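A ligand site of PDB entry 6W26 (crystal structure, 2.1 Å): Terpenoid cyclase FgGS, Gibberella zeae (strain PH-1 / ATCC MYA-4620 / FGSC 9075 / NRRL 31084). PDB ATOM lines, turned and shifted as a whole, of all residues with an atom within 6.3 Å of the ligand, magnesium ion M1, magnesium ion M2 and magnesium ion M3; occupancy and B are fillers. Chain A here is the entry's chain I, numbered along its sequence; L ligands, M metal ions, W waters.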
ATOM      1  N   PHE A  91      -1.772 -26.035  -8.520  1.00  0.00           N
ATOM      2  CA  PHE A  91      -1.024 -25.139  -7.648  1.00  0.00           C
ATOM      3  C   PHE A  91       0.165 -24.511  -8.369  1.00  0.00           C
ATOM      4  O   PHE A  91       0.423 -23.313  -8.230  1.00  0.00           O
ATOM      5  CB  PHE A  91      -0.535 -25.885  -6.399  1.00  0.00           C
ATOM      6  CG  PHE A  91      -1.489 -25.841  -5.242  1.00  0.00           C
ATOM      7  CD1 PHE A  91      -1.839 -24.628  -4.671  1.00  0.00           C
ATOM      8  CD2 PHE A  91      -2.026 -27.001  -4.741  1.00  0.00           C
ATOM      9  CE1 PHE A  91      -2.713 -24.583  -3.598  1.00  0.00           C
ATOM     10  CE2 PHE A  91      -2.909 -26.974  -3.669  1.00  0.00           C
ATOM     11  CZ  PHE A  91      -3.252 -25.764  -3.105  1.00  0.00           C
ATOM     12  N   ASP A  94      -0.937 -22.311 -11.316  1.00  0.00           N
ATOM     13  CA  ASP A  94      -1.522 -21.071 -10.827  1.00  0.00           C
ATOM     14  C   ASP A  94      -0.497 -19.944 -10.798  1.00  0.00           C
ATOM     15  O   ASP A  94      -0.775 -18.829 -11.248  1.00  0.00           O
ATOM     16  CB  ASP A  94      -2.121 -21.301  -9.435  1.00  0.00           C
ATOM     17  CG  ASP A  94      -2.408 -20.002  -8.697  1.00  0.00           C
ATOM     18  OD1 ASP A  94      -3.319 -19.262  -9.117  1.00  0.00           O
ATOM     19  OD2 ASP A  94      -1.730 -19.728  -7.672  1.00  0.00           O
ATOM     20  N   SER A  95       0.703 -20.209 -10.271  1.00  0.00           N
ATOM     21  CA  SER A  95       1.710 -19.168 -10.191  1.00  0.00           C
ATOM     22  C   SER A  95       2.243 -18.770 -11.562  1.00  0.00           C
ATOM     23  O   SER A  95       2.682 -17.634 -11.754  1.00  0.00           O
ATOM     24  CB  SER A  95       2.865 -19.606  -9.277  1.00  0.00           C
ATOM     25  OG  SER A  95       2.369 -20.013  -8.016  1.00  0.00           O
ATOM     26  N   GLU A  98      -0.141 -16.173 -12.898  1.00  0.00           N
ATOM     27  CA  GLU A  98       0.010 -14.891 -12.233  1.00  0.00           C
ATOM     28  C   GLU A  98       1.321 -14.194 -12.560  1.00  0.00           C
ATOM     29  O   GLU A  98       1.458 -13.004 -12.271  1.00  0.00           O
ATOM     30  CB  GLU A  98      -0.098 -15.082 -10.715  1.00  0.00           C
ATOM     31  CG  GLU A  98      -1.511 -15.368 -10.226  1.00  0.00           C
ATOM     32  CD  GLU A  98      -1.555 -15.747  -8.751  1.00  0.00           C
ATOM     33  OE1 GLU A  98      -1.026 -14.970  -7.922  1.00  0.00           O
ATOM     34  OE2 GLU A  98      -2.110 -16.823  -8.434  1.00  0.00           O
ATOM     35  N   THR A 147      -8.908 -16.298 -15.226  1.00  0.00           N
ATOM     36  CA  THR A 147      -7.678 -15.731 -14.698  1.00  0.00           C
ATOM     37  C   THR A 147      -6.897 -15.014 -15.795  1.00  0.00           C
ATOM     38  O   THR A 147      -6.460 -13.866 -15.624  1.00  0.00           O
ATOM     39  CB  THR A 147      -6.813 -16.828 -14.069  1.00  0.00           C
ATOM     40  OG1 THR A 147      -7.479 -17.362 -12.917  1.00  0.00           O
ATOM     41  CG2 THR A 147      -5.456 -16.283 -13.657  1.00  0.00           C
ATOM     42  N   ARG A 165     -13.015 -13.496  -8.193  1.00  0.00           N
ATOM     43  CA  ARG A 165     -12.057 -14.231  -7.369  1.00  0.00           C
ATOM     44  C   ARG A 165     -12.532 -15.642  -7.056  1.00  0.00           C
ATOM     45  O   ARG A 165     -11.719 -16.567  -6.995  1.00  0.00           O
ATOM     46  CB  ARG A 165     -11.791 -13.463  -6.078  1.00  0.00           C
ATOM     47  CG  ARG A 165     -10.742 -14.104  -5.183  1.00  0.00           C
ATOM     48  CD  ARG A 165      -9.344 -14.036  -5.803  1.00  0.00           C
ATOM     49  NE  ARG A 165      -8.353 -14.452  -4.813  1.00  0.00           N
ATOM     50  CZ  ARG A 165      -7.545 -15.501  -4.965  1.00  0.00           C
ATOM     51  NH1 ARG A 165      -7.596 -16.228  -6.073  1.00  0.00           N
ATOM     52  NH2 ARG A 165      -6.686 -15.824  -4.007  1.00  0.00           N
ATOM     53  N   ASP A 168     -11.324 -17.468  -9.998  1.00  0.00           N
ATOM     54  CA  ASP A 168      -9.868 -17.458 -10.080  1.00  0.00           C
ATOM     55  C   ASP A 168      -9.239 -18.350  -9.013  1.00  0.00           C
ATOM     56  O   ASP A 168      -8.259 -19.047  -9.281  1.00  0.00           O
ATOM     57  CB  ASP A 168      -9.357 -16.015  -9.968  1.00  0.00           C
ATOM     58  CG  ASP A 168      -7.848 -15.921  -9.798  1.00  0.00           C
ATOM     59  OD1 ASP A 168      -7.379 -15.604  -8.681  1.00  0.00           O
ATOM     60  OD2 ASP A 168      -7.112 -16.152 -10.780  1.00  0.00           O
ATOM     61  N   THR A 169      -9.784 -18.342  -7.798  1.00  0.00           N
ATOM     62  CA  THR A 169      -9.244 -19.156  -6.710  1.00  0.00           C
ATOM     63  C   THR A 169      -9.512 -20.638  -6.897  1.00  0.00           C
ATOM     64  O   THR A 169      -8.924 -21.454  -6.173  1.00  0.00           O
ATOM     65  CB  THR A 169      -9.802 -18.679  -5.372  1.00  0.00           C
ATOM     66  OG1 THR A 169      -8.887 -19.017  -4.316  1.00  0.00           O
ATOM     67  CG2 THR A 169     -11.152 -19.351  -5.084  1.00  0.00           C
ATOM     68  N   GLY A 170     -10.359 -21.023  -7.852  1.00  0.00           N
ATOM     69  CA  GLY A 170     -10.618 -22.424  -8.113  1.00  0.00           C
ATOM     70  C   GLY A 170     -11.718 -23.051  -7.297  1.00  0.00           C
ATOM     71  O   GLY A 170     -11.761 -24.283  -7.186  1.00  0.00           O
ATOM     72  N   ASN A 209      -8.095 -17.474   1.839  1.00  0.00           N
ATOM     73  CA  ASN A 209      -6.809 -17.613   1.164  1.00  0.00           C
ATOM     74  C   ASN A 209      -6.094 -16.270   1.095  1.00  0.00           C
ATOM     75  O   ASN A 209      -4.890 -16.174   1.366  1.00  0.00           O
ATOM     76  CB  ASN A 209      -6.992 -18.198  -0.232  1.00  0.00           C
ATOM     77  CG  ASN A 209      -5.679 -18.286  -0.995  1.00  0.00           C
ATOM     78  OD1 ASN A 209      -4.985 -19.298  -0.915  1.00  0.00           O
ATOM     79  ND2 ASN A 209      -5.339 -17.229  -1.707  1.00  0.00           N
ATOM     80  N   ASP A 210      -6.821 -15.201   0.722  1.00  0.00           N
ATOM     81  CA  ASP A 210      -6.241 -13.861   0.710  1.00  0.00           C
ATOM     82  C   ASP A 210      -5.590 -13.525   2.047  1.00  0.00           C
ATOM     83  O   ASP A 210      -4.475 -13.012   2.104  1.00  0.00           O
ATOM     84  CB  ASP A 210      -7.316 -12.821   0.390  1.00  0.00           C
ATOM     85  CG  ASP A 210      -7.783 -12.870  -1.051  1.00  0.00           C
ATOM     86  OD1 ASP A 210      -8.766 -12.172  -1.360  1.00  0.00           O
ATOM     87  OD2 ASP A 210      -7.171 -13.596  -1.859  1.00  0.00           O
ATOM     88  N   SER A 213      -2.354 -15.817   2.556  1.00  0.00           N
ATOM     89  CA  SER A 213      -1.343 -15.799   1.493  1.00  0.00           C
ATOM     90  C   SER A 213      -0.907 -14.396   1.126  1.00  0.00           C
ATOM     91  O   SER A 213      -0.105 -14.236   0.188  1.00  0.00           O
ATOM     92  CB  SER A 213      -1.857 -16.544   0.247  1.00  0.00           C
ATOM     93  OG  SER A 213      -2.919 -15.852  -0.391  1.00  0.00           O
ATOM     94  N   PHE A 214      -1.401 -13.359   1.824  1.00  0.00           N
ATOM     95  CA  PHE A 214      -1.075 -11.979   1.472  1.00  0.00           C
ATOM     96  C   PHE A 214       0.409 -11.691   1.646  1.00  0.00           C
ATOM     97  O   PHE A 214       1.022 -11.023   0.793  1.00  0.00           O
ATOM     98  CB  PHE A 214      -1.911 -11.017   2.329  1.00  0.00           C
ATOM     99  CG  PHE A 214      -1.554  -9.566   2.132  1.00  0.00           C
ATOM    100  CD1 PHE A 214      -2.119  -8.835   1.102  1.00  0.00           C
ATOM    101  CD2 PHE A 214      -0.645  -8.932   2.976  1.00  0.00           C
ATOM    102  CE1 PHE A 214      -1.800  -7.502   0.918  1.00  0.00           C
ATOM    103  CE2 PHE A 214      -0.326  -7.598   2.792  1.00  0.00           C
ATOM    104  CZ  PHE A 214      -0.907  -6.882   1.767  1.00  0.00           C
ATOM    105  N   ARG A 216       2.994 -13.640   1.506  1.00  0.00           N
ATOM    106  CA  ARG A 216       3.772 -14.292   0.441  1.00  0.00           C
ATOM    107  C   ARG A 216       3.524 -13.605  -0.905  1.00  0.00           C
ATOM    108  O   ARG A 216       4.423 -13.417  -1.596  1.00  0.00           O
ATOM    109  CB  ARG A 216       3.425 -15.780   0.388  1.00  0.00           C
ATOM    110  CG  ARG A 216       3.773 -16.423  -0.930  1.00  0.00           C
ATOM    111  CD  ARG A 216       2.641 -16.532  -1.920  1.00  0.00           C
ATOM    112  NE  ARG A 216       2.832 -17.643  -2.804  1.00  0.00           N
ATOM    113  CZ  ARG A 216       1.941 -18.177  -3.613  1.00  0.00           C
ATOM    114  NH1 ARG A 216       0.706 -17.719  -3.603  1.00  0.00           N
ATOM    115  NH2 ARG A 216       2.282 -19.184  -4.398  1.00  0.00           N
ATOM    116  N   GLU A 217       2.288 -13.211  -1.161  1.00  0.00           N
ATOM    117  CA  GLU A 217       1.986 -12.570  -2.436  1.00  0.00           C
ATOM    118  C   GLU A 217       2.584 -11.177  -2.516  1.00  0.00           C
ATOM    119  O   GLU A 217       2.934 -10.711  -3.605  1.00  0.00           O
ATOM    120  CB  GLU A 217       0.474 -12.556  -2.659  1.00  0.00           C
ATOM    121  CG  GLU A 217      -0.046 -13.931  -3.076  1.00  0.00           C
ATOM    122  CD  GLU A 217      -1.541 -14.096  -2.933  1.00  0.00           C
ATOM    123  OE1 GLU A 217      -2.003 -15.248  -3.036  1.00  0.00           O
ATOM    124  OE2 GLU A 217      -2.260 -13.085  -2.745  1.00  0.00           O
ATOM    125  N   ILE A 227      -3.372 -10.413  -6.558  1.00  0.00           N
ATOM    126  CA  ILE A 227      -4.817 -10.606  -6.518  1.00  0.00           C
ATOM    127  C   ILE A 227      -5.180 -10.929  -5.075  1.00  0.00           C
ATOM    128  O   ILE A 227      -5.089 -12.081  -4.640  1.00  0.00           O
ATOM    129  CB  ILE A 227      -5.267 -11.728  -7.472  1.00  0.00           C
ATOM    130  CG1 ILE A 227      -4.711 -11.475  -8.875  1.00  0.00           C
ATOM    131  CG2 ILE A 227      -6.781 -11.821  -7.507  1.00  0.00           C
ATOM    132  CD1 ILE A 227      -4.687 -12.716  -9.739  1.00  0.00           C
ATOM    133  N   ASN A 228      -5.591  -9.907  -4.312  1.00  0.00           N
ATOM    134  CA  ASN A 228      -5.795 -10.096  -2.882  1.00  0.00           C
ATOM    135  C   ASN A 228      -6.679  -9.002  -2.324  1.00  0.00           C
ATOM    136  O   ASN A 228      -6.380  -7.808  -2.480  1.00  0.00           O
ATOM    137  CB  ASN A 228      -4.457 -10.126  -2.145  1.00  0.00           C
ATOM    138  CG  ASN A 228      -4.571 -10.763  -0.780  1.00  0.00           C
ATOM    139  OD1 ASN A 228      -5.338 -10.311   0.064  1.00  0.00           O
ATOM    140  ND2 ASN A 228      -3.809 -11.836  -0.553  1.00  0.00           N
ATOM    141  N   TRP A 294      -5.140 -25.836   6.915  1.00  0.00           N
ATOM    142  CA  TRP A 294      -3.975 -26.041   6.045  1.00  0.00           C
ATOM    143  C   TRP A 294      -3.208 -24.744   5.824  1.00  0.00           C
ATOM    144  O   TRP A 294      -1.970 -24.741   5.818  1.00  0.00           O
ATOM    145  CB  TRP A 294      -4.408 -26.661   4.721  1.00  0.00           C
ATOM    146  CG  TRP A 294      -3.328 -26.646   3.672  1.00  0.00           C
ATOM    147  CD1 TRP A 294      -2.342 -27.571   3.503  1.00  0.00           C
ATOM    148  CD2 TRP A 294      -3.139 -25.652   2.657  1.00  0.00           C
ATOM    149  NE1 TRP A 294      -1.541 -27.206   2.438  1.00  0.00           N
ATOM    150  CE2 TRP A 294      -2.016 -26.038   1.904  1.00  0.00           C
ATOM    151  CE3 TRP A 294      -3.807 -24.469   2.309  1.00  0.00           C
ATOM    152  CZ2 TRP A 294      -1.541 -25.288   0.832  1.00  0.00           C
ATOM    153  CZ3 TRP A 294      -3.338 -23.729   1.250  1.00  0.00           C
ATOM    154  CH2 TRP A 294      -2.213 -24.140   0.511  1.00  0.00           C
ATOM    155  N   ARG A 300       3.776 -23.272   1.509  1.00  0.00           N
ATOM    156  CA  ARG A 300       3.501 -22.388   0.381  1.00  0.00           C
ATOM    157  C   ARG A 300       3.439 -20.928   0.809  1.00  0.00           C
ATOM    158  O   ARG A 300       3.993 -20.053   0.134  1.00  0.00           O
ATOM    159  CB  ARG A 300       2.202 -22.812  -0.319  1.00  0.00           C
ATOM    160  CG  ARG A 300       1.923 -22.089  -1.639  1.00  0.00           C
ATOM    161  CD  ARG A 300       0.704 -22.679  -2.329  1.00  0.00           C
ATOM    162  NE  ARG A 300       0.253 -21.904  -3.488  1.00  0.00           N
ATOM    163  CZ  ARG A 300       0.706 -22.077  -4.726  1.00  0.00           C
ATOM    164  NH1 ARG A 300       1.621 -23.001  -4.989  1.00  0.00           N
ATOM    165  NH2 ARG A 300       0.228 -21.327  -5.718  1.00  0.00           N
ATOM    166  N   TYR A 301       2.773 -20.633   1.928  1.00  0.00           N
ATOM    167  CA  TYR A 301       2.620 -19.263   2.392  1.00  0.00           C
ATOM    168  C   TYR A 301       3.520 -18.893   3.566  1.00  0.00           C
ATOM    169  O   TYR A 301       3.579 -17.715   3.932  1.00  0.00           O
ATOM    170  CB  TYR A 301       1.157 -18.973   2.791  1.00  0.00           C
ATOM    171  CG  TYR A 301       0.094 -19.494   1.835  1.00  0.00           C
ATOM    172  CD1 TYR A 301       0.333 -19.577   0.463  1.00  0.00           C
ATOM    173  CD2 TYR A 301      -1.152 -19.876   2.303  1.00  0.00           C
ATOM    174  CE1 TYR A 301      -0.641 -20.051  -0.403  1.00  0.00           C
ATOM    175  CE2 TYR A 301      -2.133 -20.348   1.443  1.00  0.00           C
ATOM    176  CZ  TYR A 301      -1.866 -20.435   0.088  1.00  0.00           C
ATOM    177  OH  TYR A 301      -2.832 -20.905  -0.755  1.00  0.00           O
HETATM  178  P1  LIG L   1      -2.467 -19.323  -3.665  1.00  0.00           P
HETATM  179  O1  LIG L   1      -2.220 -20.684  -3.072  1.00  0.00           O
HETATM  180  O2  LIG L   1      -2.646 -18.318  -2.564  1.00  0.00           O
HETATM  181  O3  LIG L   1      -1.329 -18.912  -4.556  1.00  0.00           O
HETATM  182  O4  LIG L   1      -3.814 -19.410  -4.543  1.00  0.00           O
HETATM  183  P2  LIG L   1      -4.508 -18.116  -5.202  1.00  0.00           P
HETATM  184  O5  LIG L   1      -4.283 -16.890  -4.354  1.00  0.00           O
HETATM  185  O6  LIG L   1      -5.983 -18.400  -5.354  1.00  0.00           O
HETATM  186  O7  LIG L   1      -3.865 -17.914  -6.548  1.00  0.00           O
HETATM  187 MG    MG M   1      -1.724 -17.960  -6.449  1.00  0.00          MG
HETATM  188 MG    MG M   2      -4.098 -17.440  -8.584  1.00  0.00          MG
HETATM  189 MG    MG M   3      -3.530 -16.439  -2.403  1.00  0.00          MG
HETATM  190  O   HOH W   1      -4.531 -14.588  -2.619  1.00  0.00           O
HETATM  191  O   HOH W   2      -4.697 -16.930 -10.538  1.00  0.00           O
HETATM  192  O   HOH W   3      -4.693 -15.608  -8.072  1.00  0.00           O
HETATM  193  O   HOH W   4       0.417 -18.112  -6.903  1.00  0.00           O
HETATM  194  O   HOH W   5      -1.069 -16.124  -5.558  1.00  0.00           O
HETATM  195  O   HOH W   6      -4.105 -14.561  -5.789  1.00  0.00           O
HETATM  196  O   HOH W   7      -5.949 -18.483  -8.201  1.00  0.00           O
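OE1 of Glu 217 sits close to NH1 of Arg 216 (3.7 Å). OE2 of Glu 217 sits at hydrogen-bond distance from ND2 of Asn 228 (3.0 Å). The side-chain carboxylate of Asp 94 sits close to the guanidinium group of Arg 300 (3.2 Å). The side-chain hydroxyl (OH) of Tyr 301 sits at hydrogen-bond distance from the side-chain amide oxygen (OD1) of Asn 209. OD1 of Asp 168 lies within salt-bridge range of NH1 of Arg 165, at 2.7 Å. NH2 of Arg 165 is in salt-bridge range of OD2 of Asp 210, at 3.1 Å. NH2 of Arg 300 lies within hydrogen-bond range of OG of Ser 95. OG1 of Thr 147 lies within hydrogen-bond range of OD2 of Asp 168.
Merely in contact with magnesium ion M3: Arg 165 (3.6 Å). Four residues have an atom within 4 Å of magnesium ion M3: Arg 165, Asn 209, Ser 213 and Glu 217. The nearest printed residue that does not touch magnesium ion M3 is Arg 216 (4.6 Å).
The side-chain hydroxyl (OH) of Tyr 301 sits at hydrogen-bond distance from an oxygen (O1) of the ligand (2.4 Å). NH1 of Arg 216 sits close to O3 of the ligand. An oxygen (O6) of the ligand is in salt-bridge range of the guanidinium group of Arg 165 (2.8 Å). NE of Arg 300 lies within salt-bridge range of O1 of the ligand (2.8 Å). OG1 of Thr 169 sits at hydrogen-bond distance from O6 of the ligand, 3.1 Å away.
Magnesium ion M3 is bound by OE1 of Glu 217 (2.0 Å), O2 of the ligand (2.1 Å), ND2 of Asn 209 (2.1 Å), water W1 (2.1 Å), O5 of the ligand (2.1 Å) and OG of Ser 213 (2.2 Å).
Residues that only touch magnesium ion M1: Arg 216 (3.8 Å) and Arg 300 (3.96 Å). The nearest printed residue that does not touch magnesium ion M1 is Glu 217 (4.4 Å).
Magnesium ion M2 is bound by water W3 (2.0 Å), the side-chain carboxylate of Asp 94 (2.1 Å), the side-chain carboxylate of Glu 98 (2.1 Å), an oxygen (O7) of the ligand (2.1 Å), water W2 (2.1 Å) and water W7 (2.2 Å). Magnesium ion M2 has six donor atoms within binding distance.
Phe 91 touches the ligand (CE1 to O1, 3.97 Å). Hydrophobic or aromatic side chains that line the ligand: Phe 91 and Tyr 301. 11 residues have an atom within 4 Å of the ligand: Phe 91, Asp 94, Glu 98, Arg 165, Thr 169, Asn 209, Ser 213, Arg 216, Glu 217, Arg 300 and Tyr 301. The nearest printed residue that does not touch the ligand is Asp 168 (4.6 Å).
Magnesium ion M1 is bound by O7 of the ligand (2.1 Å), water W5 (2.1 Å), OD2 of Asp 94 (2.1 Å), O3 of the ligand (2.2 Å), water W4 (2.2 Å) and OE2 of Glu 98 (2.3 Å).
Residues that only touch magnesium ion M2: Asp 168 (3.8 Å). Of the 20 residues printed, 3 come within 4 Å of magnesium ion M2.
Water W5 lies within hydrogen-bond range of the side-chain carboxylate of Glu 98 (2.6 Å) and the guanidinium group of Arg 216 (3.1 Å). Water W4 lies within hydrogen-bond range of the side-chain hydroxyl (OG) of Ser 95 (2.9 Å), the guanidinium group (NH2) of Arg 216 (3.3 Å) and the guanidinium group (NH2) of Arg 300 (3.4 Å). Water W7 bridges O of Asp 168 and O6 of the ligand. Water W6 lies within hydrogen-bond range of the backbone carbonyl oxygen (O) of Ile 227 (2.9 Å) and the guanidinium group (NH2) of Arg 165 (3.4 Å).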
